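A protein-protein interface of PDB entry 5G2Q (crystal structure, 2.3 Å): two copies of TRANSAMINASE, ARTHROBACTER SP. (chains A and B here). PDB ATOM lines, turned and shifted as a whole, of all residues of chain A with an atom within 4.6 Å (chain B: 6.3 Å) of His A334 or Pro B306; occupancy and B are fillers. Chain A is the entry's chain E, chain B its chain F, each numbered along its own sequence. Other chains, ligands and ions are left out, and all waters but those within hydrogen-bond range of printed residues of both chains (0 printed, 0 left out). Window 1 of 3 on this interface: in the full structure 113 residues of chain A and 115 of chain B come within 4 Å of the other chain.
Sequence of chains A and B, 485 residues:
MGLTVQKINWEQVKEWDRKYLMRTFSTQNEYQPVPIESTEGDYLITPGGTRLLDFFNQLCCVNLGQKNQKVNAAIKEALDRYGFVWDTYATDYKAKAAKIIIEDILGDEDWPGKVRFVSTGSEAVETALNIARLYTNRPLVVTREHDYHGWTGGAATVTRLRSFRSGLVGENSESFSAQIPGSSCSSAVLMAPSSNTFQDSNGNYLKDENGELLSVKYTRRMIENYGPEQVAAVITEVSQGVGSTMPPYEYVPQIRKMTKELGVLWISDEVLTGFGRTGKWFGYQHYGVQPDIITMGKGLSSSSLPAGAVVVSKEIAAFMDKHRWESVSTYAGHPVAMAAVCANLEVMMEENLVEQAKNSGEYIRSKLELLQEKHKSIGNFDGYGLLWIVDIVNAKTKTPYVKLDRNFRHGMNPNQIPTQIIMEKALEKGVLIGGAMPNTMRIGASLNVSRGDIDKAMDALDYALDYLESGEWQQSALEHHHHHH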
ATOM      1  N   GLY A  83       3.937  -1.328 -29.411  1.00  0.00           N
ATOM      2  CA  GLY A  83       3.948  -2.687 -29.928  1.00  0.00           C
ATOM      3  C   GLY A  83       5.350  -3.186 -29.939  1.00  0.00           C
ATOM      4  O   GLY A  83       6.250  -2.481 -29.493  1.00  0.00           O
ATOM      5  N   PHE A  84       5.551  -4.386 -30.472  1.00  0.00           N
ATOM      6  CA  PHE A  84       6.878  -5.028 -30.508  1.00  0.00           C
ATOM      7  C   PHE A  84       7.101  -5.983 -31.707  1.00  0.00           C
ATOM      8  O   PHE A  84       6.271  -6.861 -31.976  1.00  0.00           O
ATOM      9  CB  PHE A  84       7.126  -5.779 -29.190  1.00  0.00           C
ATOM     10  CG  PHE A  84       8.259  -6.749 -29.266  1.00  0.00           C
ATOM     11  CD1 PHE A  84       9.563  -6.298 -29.262  1.00  0.00           C
ATOM     12  CD2 PHE A  84       8.021  -8.123 -29.414  1.00  0.00           C
ATOM     13  CE1 PHE A  84      10.617  -7.189 -29.378  1.00  0.00           C
ATOM     14  CE2 PHE A  84       9.084  -9.023 -29.521  1.00  0.00           C
ATOM     15  CZ  PHE A  84      10.383  -8.551 -29.504  1.00  0.00           C
ATOM     16  N   SER A 119      20.218  -5.356 -26.014  1.00  0.00           N
ATOM     17  CA  SER A 119      19.570  -4.531 -24.975  1.00  0.00           C
ATOM     18  C   SER A 119      20.530  -3.852 -23.968  1.00  0.00           C
ATOM     19  O   SER A 119      20.199  -2.839 -23.369  1.00  0.00           O
ATOM     20  CB  SER A 119      18.477  -5.334 -24.270  1.00  0.00           C
ATOM     21  OG  SER A 119      17.499  -5.704 -25.216  1.00  0.00           O
ATOM     22  N   PRO A 306      16.760   0.982 -22.692  1.00  0.00           N
ATOM     23  CA  PRO A 306      17.955   0.128 -22.752  1.00  0.00           C
ATOM     24  C   PRO A 306      18.284  -0.260 -24.175  1.00  0.00           C
ATOM     25  O   PRO A 306      17.429  -0.847 -24.873  1.00  0.00           O
ATOM     26  CB  PRO A 306      17.567  -1.147 -21.974  1.00  0.00           C
ATOM     27  CG  PRO A 306      16.178  -0.949 -21.462  1.00  0.00           C
ATOM     28  CD  PRO A 306      15.666   0.407 -21.879  1.00  0.00           C
ATOM     29  N   TYR A 331      14.484  -9.302 -27.296  1.00  0.00           N
ATOM     30  CA  TYR A 331      14.341  -7.847 -27.429  1.00  0.00           C
ATOM     31  C   TYR A 331      15.394  -7.166 -28.278  1.00  0.00           C
ATOM     32  O   TYR A 331      15.411  -5.940 -28.378  1.00  0.00           O
ATOM     33  CB  TYR A 331      14.355  -7.176 -26.062  1.00  0.00           C
ATOM     34  CG  TYR A 331      13.263  -7.643 -25.148  1.00  0.00           C
ATOM     35  CD1 TYR A 331      11.948  -7.824 -25.610  1.00  0.00           C
ATOM     36  CD2 TYR A 331      13.540  -7.910 -23.814  1.00  0.00           C
ATOM     37  CE1 TYR A 331      10.945  -8.264 -24.753  1.00  0.00           C
ATOM     38  CE2 TYR A 331      12.545  -8.343 -22.949  1.00  0.00           C
ATOM     39  CZ  TYR A 331      11.254  -8.512 -23.407  1.00  0.00           C
ATOM     40  OH  TYR A 331      10.301  -8.932 -22.494  1.00  0.00           O
ATOM     41  N   ALA A 332      16.271  -7.953 -28.882  1.00  0.00           N
ATOM     42  CA  ALA A 332      17.297  -7.412 -29.748  1.00  0.00           C
ATOM     43  C   ALA A 332      16.592  -6.677 -30.856  1.00  0.00           C
ATOM     44  O   ALA A 332      15.844  -7.282 -31.612  1.00  0.00           O
ATOM     45  CB  ALA A 332      18.162  -8.534 -30.324  1.00  0.00           C
ATOM     46  N   GLY A 333      16.811  -5.375 -30.931  1.00  0.00           N
ATOM     47  CA  GLY A 333      16.288  -4.553 -32.011  1.00  0.00           C
ATOM     48  C   GLY A 333      14.960  -3.921 -31.713  1.00  0.00           C
ATOM     49  O   GLY A 333      14.384  -3.261 -32.584  1.00  0.00           O
ATOM     50  N   HIS A 334      14.501  -4.103 -30.472  1.00  0.00           N
ATOM     51  CA  HIS A 334      13.212  -3.554 -30.003  1.00  0.00           C
ATOM     52  C   HIS A 334      12.881  -2.217 -30.644  1.00  0.00           C
ATOM     53  O   HIS A 334      13.584  -1.240 -30.423  1.00  0.00           O
ATOM     54  CB  HIS A 334      13.218  -3.386 -28.486  1.00  0.00           C
ATOM     55  CG  HIS A 334      11.857  -3.301 -27.885  1.00  0.00           C
ATOM     56  ND1 HIS A 334      10.997  -2.251 -28.134  1.00  0.00           N
ATOM     57  CD2 HIS A 334      11.189  -4.143 -27.063  1.00  0.00           C
ATOM     58  CE1 HIS A 334       9.865  -2.439 -27.478  1.00  0.00           C
ATOM     59  NE2 HIS A 334       9.948  -3.586 -26.833  1.00  0.00           N
ATOM     60  N   PRO A 335      11.786  -2.157 -31.419  1.00  0.00           N
ATOM     61  CA  PRO A 335      11.445  -0.974 -32.225  1.00  0.00           C
ATOM     62  C   PRO A 335      11.344   0.357 -31.474  1.00  0.00           C
ATOM     63  O   PRO A 335      11.729   1.399 -32.033  1.00  0.00           O
ATOM     64  CB  PRO A 335      10.099  -1.344 -32.874  1.00  0.00           C
ATOM     65  CG  PRO A 335       9.699  -2.657 -32.299  1.00  0.00           C
ATOM     66  CD  PRO A 335      10.925  -3.306 -31.749  1.00  0.00           C
ATOM     67  N   VAL A 336      10.819   0.342 -30.245  1.00  0.00           N
ATOM     68  CA  VAL A 336      10.755   1.583 -29.438  1.00  0.00           C
ATOM     69  C   VAL A 336      12.157   1.971 -28.969  1.00  0.00           C
ATOM     70  O   VAL A 336      12.525   3.136 -29.027  1.00  0.00           O
ATOM     71  CB  VAL A 336       9.786   1.479 -28.228  1.00  0.00           C
ATOM     72  CG1 VAL A 336       9.509   2.853 -27.627  1.00  0.00           C
ATOM     73  CG2 VAL A 336       8.500   0.740 -28.619  1.00  0.00           C
ATOM     74  N   ALA A 337      12.941   0.973 -28.543  1.00  0.00           N
ATOM     75  CA  ALA A 337      14.362   1.165 -28.194  1.00  0.00           C
ATOM     76  C   ALA A 337      15.114   1.819 -29.365  1.00  0.00           C
ATOM     77  O   ALA A 337      15.928   2.723 -29.151  1.00  0.00           O
ATOM     78  CB  ALA A 337      15.004  -0.153 -27.794  1.00  0.00           C
ATOM     79  N   MET A 338      14.812   1.407 -30.602  1.00  0.00           N
ATOM     80  CA  MET A 338      15.474   2.014 -31.764  1.00  0.00           C
ATOM     81  C   MET A 338      15.032   3.452 -32.058  1.00  0.00           C
ATOM     82  O   MET A 338      15.852   4.278 -32.442  1.00  0.00           O
ATOM     83  CB  MET A 338      15.396   1.132 -33.011  1.00  0.00           C
ATOM     84  CG  MET A 338      15.962  -0.291 -32.850  1.00  0.00           C
ATOM     85  SD  MET A 338      17.710  -0.366 -32.404  1.00  0.00           S
ATOM     86  CE  MET A 338      17.665  -0.343 -30.611  1.00  0.00           C
ATOM     87  N   VAL B 118      16.141  -7.037 -14.365  1.00  0.00           N
ATOM     88  CA  VAL B 118      17.169  -6.787 -15.375  1.00  0.00           C
ATOM     89  C   VAL B 118      16.492  -6.397 -16.690  1.00  0.00           C
ATOM     90  O   VAL B 118      15.323  -6.049 -16.687  1.00  0.00           O
ATOM     91  CB  VAL B 118      18.119  -7.980 -15.547  1.00  0.00           C
ATOM     92  CG1 VAL B 118      19.087  -8.080 -14.369  1.00  0.00           C
ATOM     93  CG2 VAL B 118      17.328  -9.275 -15.767  1.00  0.00           C
ATOM     94  N   SER B 119      17.192  -6.480 -17.819  1.00  0.00           N
ATOM     95  CA  SER B 119      16.598  -6.027 -19.076  1.00  0.00           C
ATOM     96  C   SER B 119      16.099  -7.169 -19.987  1.00  0.00           C
ATOM     97  O   SER B 119      15.127  -6.994 -20.750  1.00  0.00           O
ATOM     98  CB  SER B 119      17.571  -5.109 -19.804  1.00  0.00           C
ATOM     99  OG  SER B 119      17.948  -4.017 -18.954  1.00  0.00           O
ATOM    100  N   THR B 120      16.745  -8.335 -19.909  1.00  0.00           N
ATOM    101  CA  THR B 120      16.356  -9.445 -20.765  1.00  0.00           C
ATOM    102  C   THR B 120      16.153 -10.725 -19.992  1.00  0.00           C
ATOM    103  O   THR B 120      16.492 -10.800 -18.804  1.00  0.00           O
ATOM    104  CB  THR B 120      17.388  -9.721 -21.856  1.00  0.00           C
ATOM    105  OG1 THR B 120      18.606 -10.201 -21.241  1.00  0.00           O
ATOM    106  CG2 THR B 120      17.630  -8.461 -22.684  1.00  0.00           C
ATOM    107  N   SER B 301       6.617  -7.851 -19.346  1.00  0.00           N
ATOM    108  CA  SER B 301       6.183  -6.570 -19.904  1.00  0.00           C
ATOM    109  C   SER B 301       5.383  -6.735 -21.196  1.00  0.00           C
ATOM    110  O   SER B 301       5.140  -5.766 -21.860  1.00  0.00           O
ATOM    111  CB  SER B 301       7.394  -5.644 -20.158  1.00  0.00           C
ATOM    112  OG  SER B 301       8.208  -6.095 -21.251  1.00  0.00           O
ATOM    113  N   SER B 303       6.524  -7.550 -23.789  1.00  0.00           N
ATOM    114  CA  SER B 303       7.485  -7.003 -24.737  1.00  0.00           C
ATOM    115  C   SER B 303       7.302  -5.515 -24.999  1.00  0.00           C
ATOM    116  O   SER B 303       7.859  -4.973 -25.956  1.00  0.00           O
ATOM    117  CB  SER B 303       7.435  -7.766 -26.061  1.00  0.00           C
ATOM    118  OG  SER B 303       7.671  -9.146 -25.861  1.00  0.00           O
ATOM    119  N   SER B 304       6.547  -4.834 -24.146  1.00  0.00           N
ATOM    120  CA  SER B 304       6.293  -3.413 -24.400  1.00  0.00           C
ATOM    121  C   SER B 304       7.600  -2.627 -24.319  1.00  0.00           C
ATOM    122  O   SER B 304       7.792  -1.694 -25.074  1.00  0.00           O
ATOM    123  CB  SER B 304       5.212  -2.845 -23.478  1.00  0.00           C
ATOM    124  OG  SER B 304       5.515  -3.101 -22.120  1.00  0.00           O
ATOM    125  N   LEU B 305       8.489  -3.040 -23.424  1.00  0.00           N
ATOM    126  CA  LEU B 305       9.841  -2.500 -23.338  1.00  0.00           C
ATOM    127  C   LEU B 305      10.731  -3.597 -22.797  1.00  0.00           C
ATOM    128  O   LEU B 305      10.203  -4.530 -22.175  1.00  0.00           O
ATOM    129  CB  LEU B 305       9.895  -1.305 -22.392  1.00  0.00           C
ATOM    130  CG  LEU B 305       9.504   0.026 -23.031  1.00  0.00           C
ATOM    131  CD1 LEU B 305       9.560   1.120 -21.978  1.00  0.00           C
ATOM    132  CD2 LEU B 305      10.398   0.340 -24.227  1.00  0.00           C
ATOM    133  N   PRO B 306      12.076  -3.500 -23.010  1.00  0.00           N
ATOM    134  CA  PRO B 306      12.969  -4.597 -22.544  1.00  0.00           C
ATOM    135  C   PRO B 306      12.976  -4.746 -21.026  1.00  0.00           C
ATOM    136  O   PRO B 306      13.285  -3.783 -20.322  1.00  0.00           O
ATOM    137  CB  PRO B 306      14.352  -4.161 -23.050  1.00  0.00           C
ATOM    138  CG  PRO B 306      14.039  -3.371 -24.277  1.00  0.00           C
ATOM    139  CD  PRO B 306      12.831  -2.544 -23.850  1.00  0.00           C
ATOM    140  N   ALA B 307      12.615  -5.939 -20.540  1.00  0.00           N
ATOM    141  CA  ALA B 307      12.477  -6.203 -19.101  1.00  0.00           C
ATOM    142  C   ALA B 307      12.699  -7.665 -18.702  1.00  0.00           C
ATOM    143  O   ALA B 307      12.022  -8.573 -19.193  1.00  0.00           O
ATOM    144  CB  ALA B 307      11.117  -5.726 -18.608  1.00  0.00           C
ATOM    145  N   GLY B 308      13.618  -7.895 -17.773  1.00  0.00           N
ATOM    146  CA  GLY B 308      13.858  -9.268 -17.263  1.00  0.00           C
ATOM    147  C   GLY B 308      13.698  -9.298 -15.756  1.00  0.00           C
ATOM    148  O   GLY B 308      13.730  -8.242 -15.103  1.00  0.00           O
ATOM    149  N   HIS B 334      15.452   0.094 -14.807  1.00  0.00           N
ATOM    150  CA  HIS B 334      15.122   1.281 -15.596  1.00  0.00           C
ATOM    151  C   HIS B 334      13.673   1.702 -15.310  1.00  0.00           C
ATOM    152  O   HIS B 334      12.745   0.923 -15.577  1.00  0.00           O
ATOM    153  CB  HIS B 334      15.294   0.921 -17.077  1.00  0.00           C
ATOM    154  CG  HIS B 334      15.403   2.102 -17.987  1.00  0.00           C
ATOM    155  ND1 HIS B 334      14.396   3.038 -18.124  1.00  0.00           N
ATOM    156  CD2 HIS B 334      16.376   2.469 -18.850  1.00  0.00           C
ATOM    157  CE1 HIS B 334      14.759   3.942 -19.017  1.00  0.00           C
ATOM    158  NE2 HIS B 334      15.959   3.618 -19.469  1.00  0.00           N
ATOM    159  N   ALA B 337      10.940   1.269 -18.240  1.00  0.00           N
ATOM    160  CA  ALA B 337      10.673  -0.166 -18.394  1.00  0.00           C
ATOM    161  C   ALA B 337       9.867  -0.678 -17.207  1.00  0.00           C
ATOM    162  O   ALA B 337       8.961  -1.479 -17.399  1.00  0.00           O
ATOM    163  CB  ALA B 337      11.954  -0.995 -18.597  1.00  0.00           C
ATOM    164  N   MET B 338      10.156  -0.184 -15.999  1.00  0.00           N
ATOM    165  CA  MET B 338       9.432  -0.622 -14.789  1.00  0.00           C
ATOM    166  C   MET B 338       7.952  -0.222 -14.781  1.00  0.00           C
ATOM    167  O   MET B 338       7.053  -0.987 -14.348  1.00  0.00           O
ATOM    168  CB  MET B 338      10.114  -0.100 -13.526  1.00  0.00           C
ATOM    169  CG  MET B 338      11.358  -0.870 -13.116  1.00  0.00           C
ATOM    170  SD  MET B 338      11.243  -2.679 -13.062  1.00  0.00           S
ATOM    171  CE  MET B 338      11.633  -3.064 -14.765  1.00  0.00           C
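A ring nitrogen (NE2) of His A334 sits at hydrogen-bond distance from the backbone carbonyl oxygen (O) of Ser B303 (2.7 Å). A ring nitrogen (NE2) of His A334 sits close to the backbone carbonyl oxygen (O) of Ser B304, at 3.4 Å.
ND1 of His A334 sits close to N of Val A336, at 3.3 Å. The backbone carbonyl oxygen (O) of Ser B119 lies within hydrogen-bond range of the backbone NH (N) of Ala B307. O of Ser B119 lies close to N of Gly B308, at 3.5 Å. N of Ser B303 sits close to OG of Ser B301. The backbone carbonyl oxygen of Ser B301 lies within hydrogen-bond range of the side-chain hydroxyl of Ser B304 (2.7 Å). The side-chain hydroxyl (OG) of Ser B301 lies within hydrogen-bond range of the backbone carbonyl oxygen (O) of Leu B305, at 2.7 Å.
Among the printed residues, merely in contact across the chains: Phe A84 with Ser B303, Ser A119 with Thr B120, Pro A306 with His B334, Tyr A331 with Ser B119, Tyr A331 with Ser B301, Tyr A331 with Ser B303, Tyr A331 with Pro B306, Tyr A331 with Ala B307, His A334 with Leu B305 and His A334 with Pro B306.
Pro A306 touches His B334, and with the chains exchanged His A334 touches Pro B306. Positions printed for both chains: 119, 306, 334, 337 and 338. Of the 12 pairs that touch across the chains among the printed residues, 2 have their exchanged pair printed and touching as well.
Of the printed residues of chain B, Pro A306 touches His B334 (3.7 Å). Of the printed residues of chain B, Tyr A331 touches Ser B119 (3.6 Å), Ser B301 (3.7 Å), Ser B303 (3.6 Å), Pro B306 (3.6 Å) and Ala B307 (3.4 Å). Of the printed residues of chain B, His A334 touches Ser B303, Ser B304, Leu B305 and Pro B306. Ala A337 touches none of the printed residues of chain B. Met A338 touches none of the printed residues of chain B. Printed residues of chain A within 4 Å of Ser B119: Tyr A331 (3.6 Å). Of the printed residues of chain A, Pro B306 touches Tyr A331 (3.6 Å) and His A334 (3.9 Å). The nearest residue of chain A that does not touch Pro B306 is Pro A306 (4.02 Å). The nearest printed residue of chain B that does not touch Pro A306 is Pro B306 (4.02 Å).
Printed residues of chain A that touch a printed residue of chain B: Phe A84, Ser A119, Pro A306, Tyr A331 and His A334. Among the printed residues, 12 pairs touch across the chains. Among the printed residues, no Asp or Glu carboxylate lies within 4 Å of a Lys or Arg side-chain nitrogen of the other chain.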
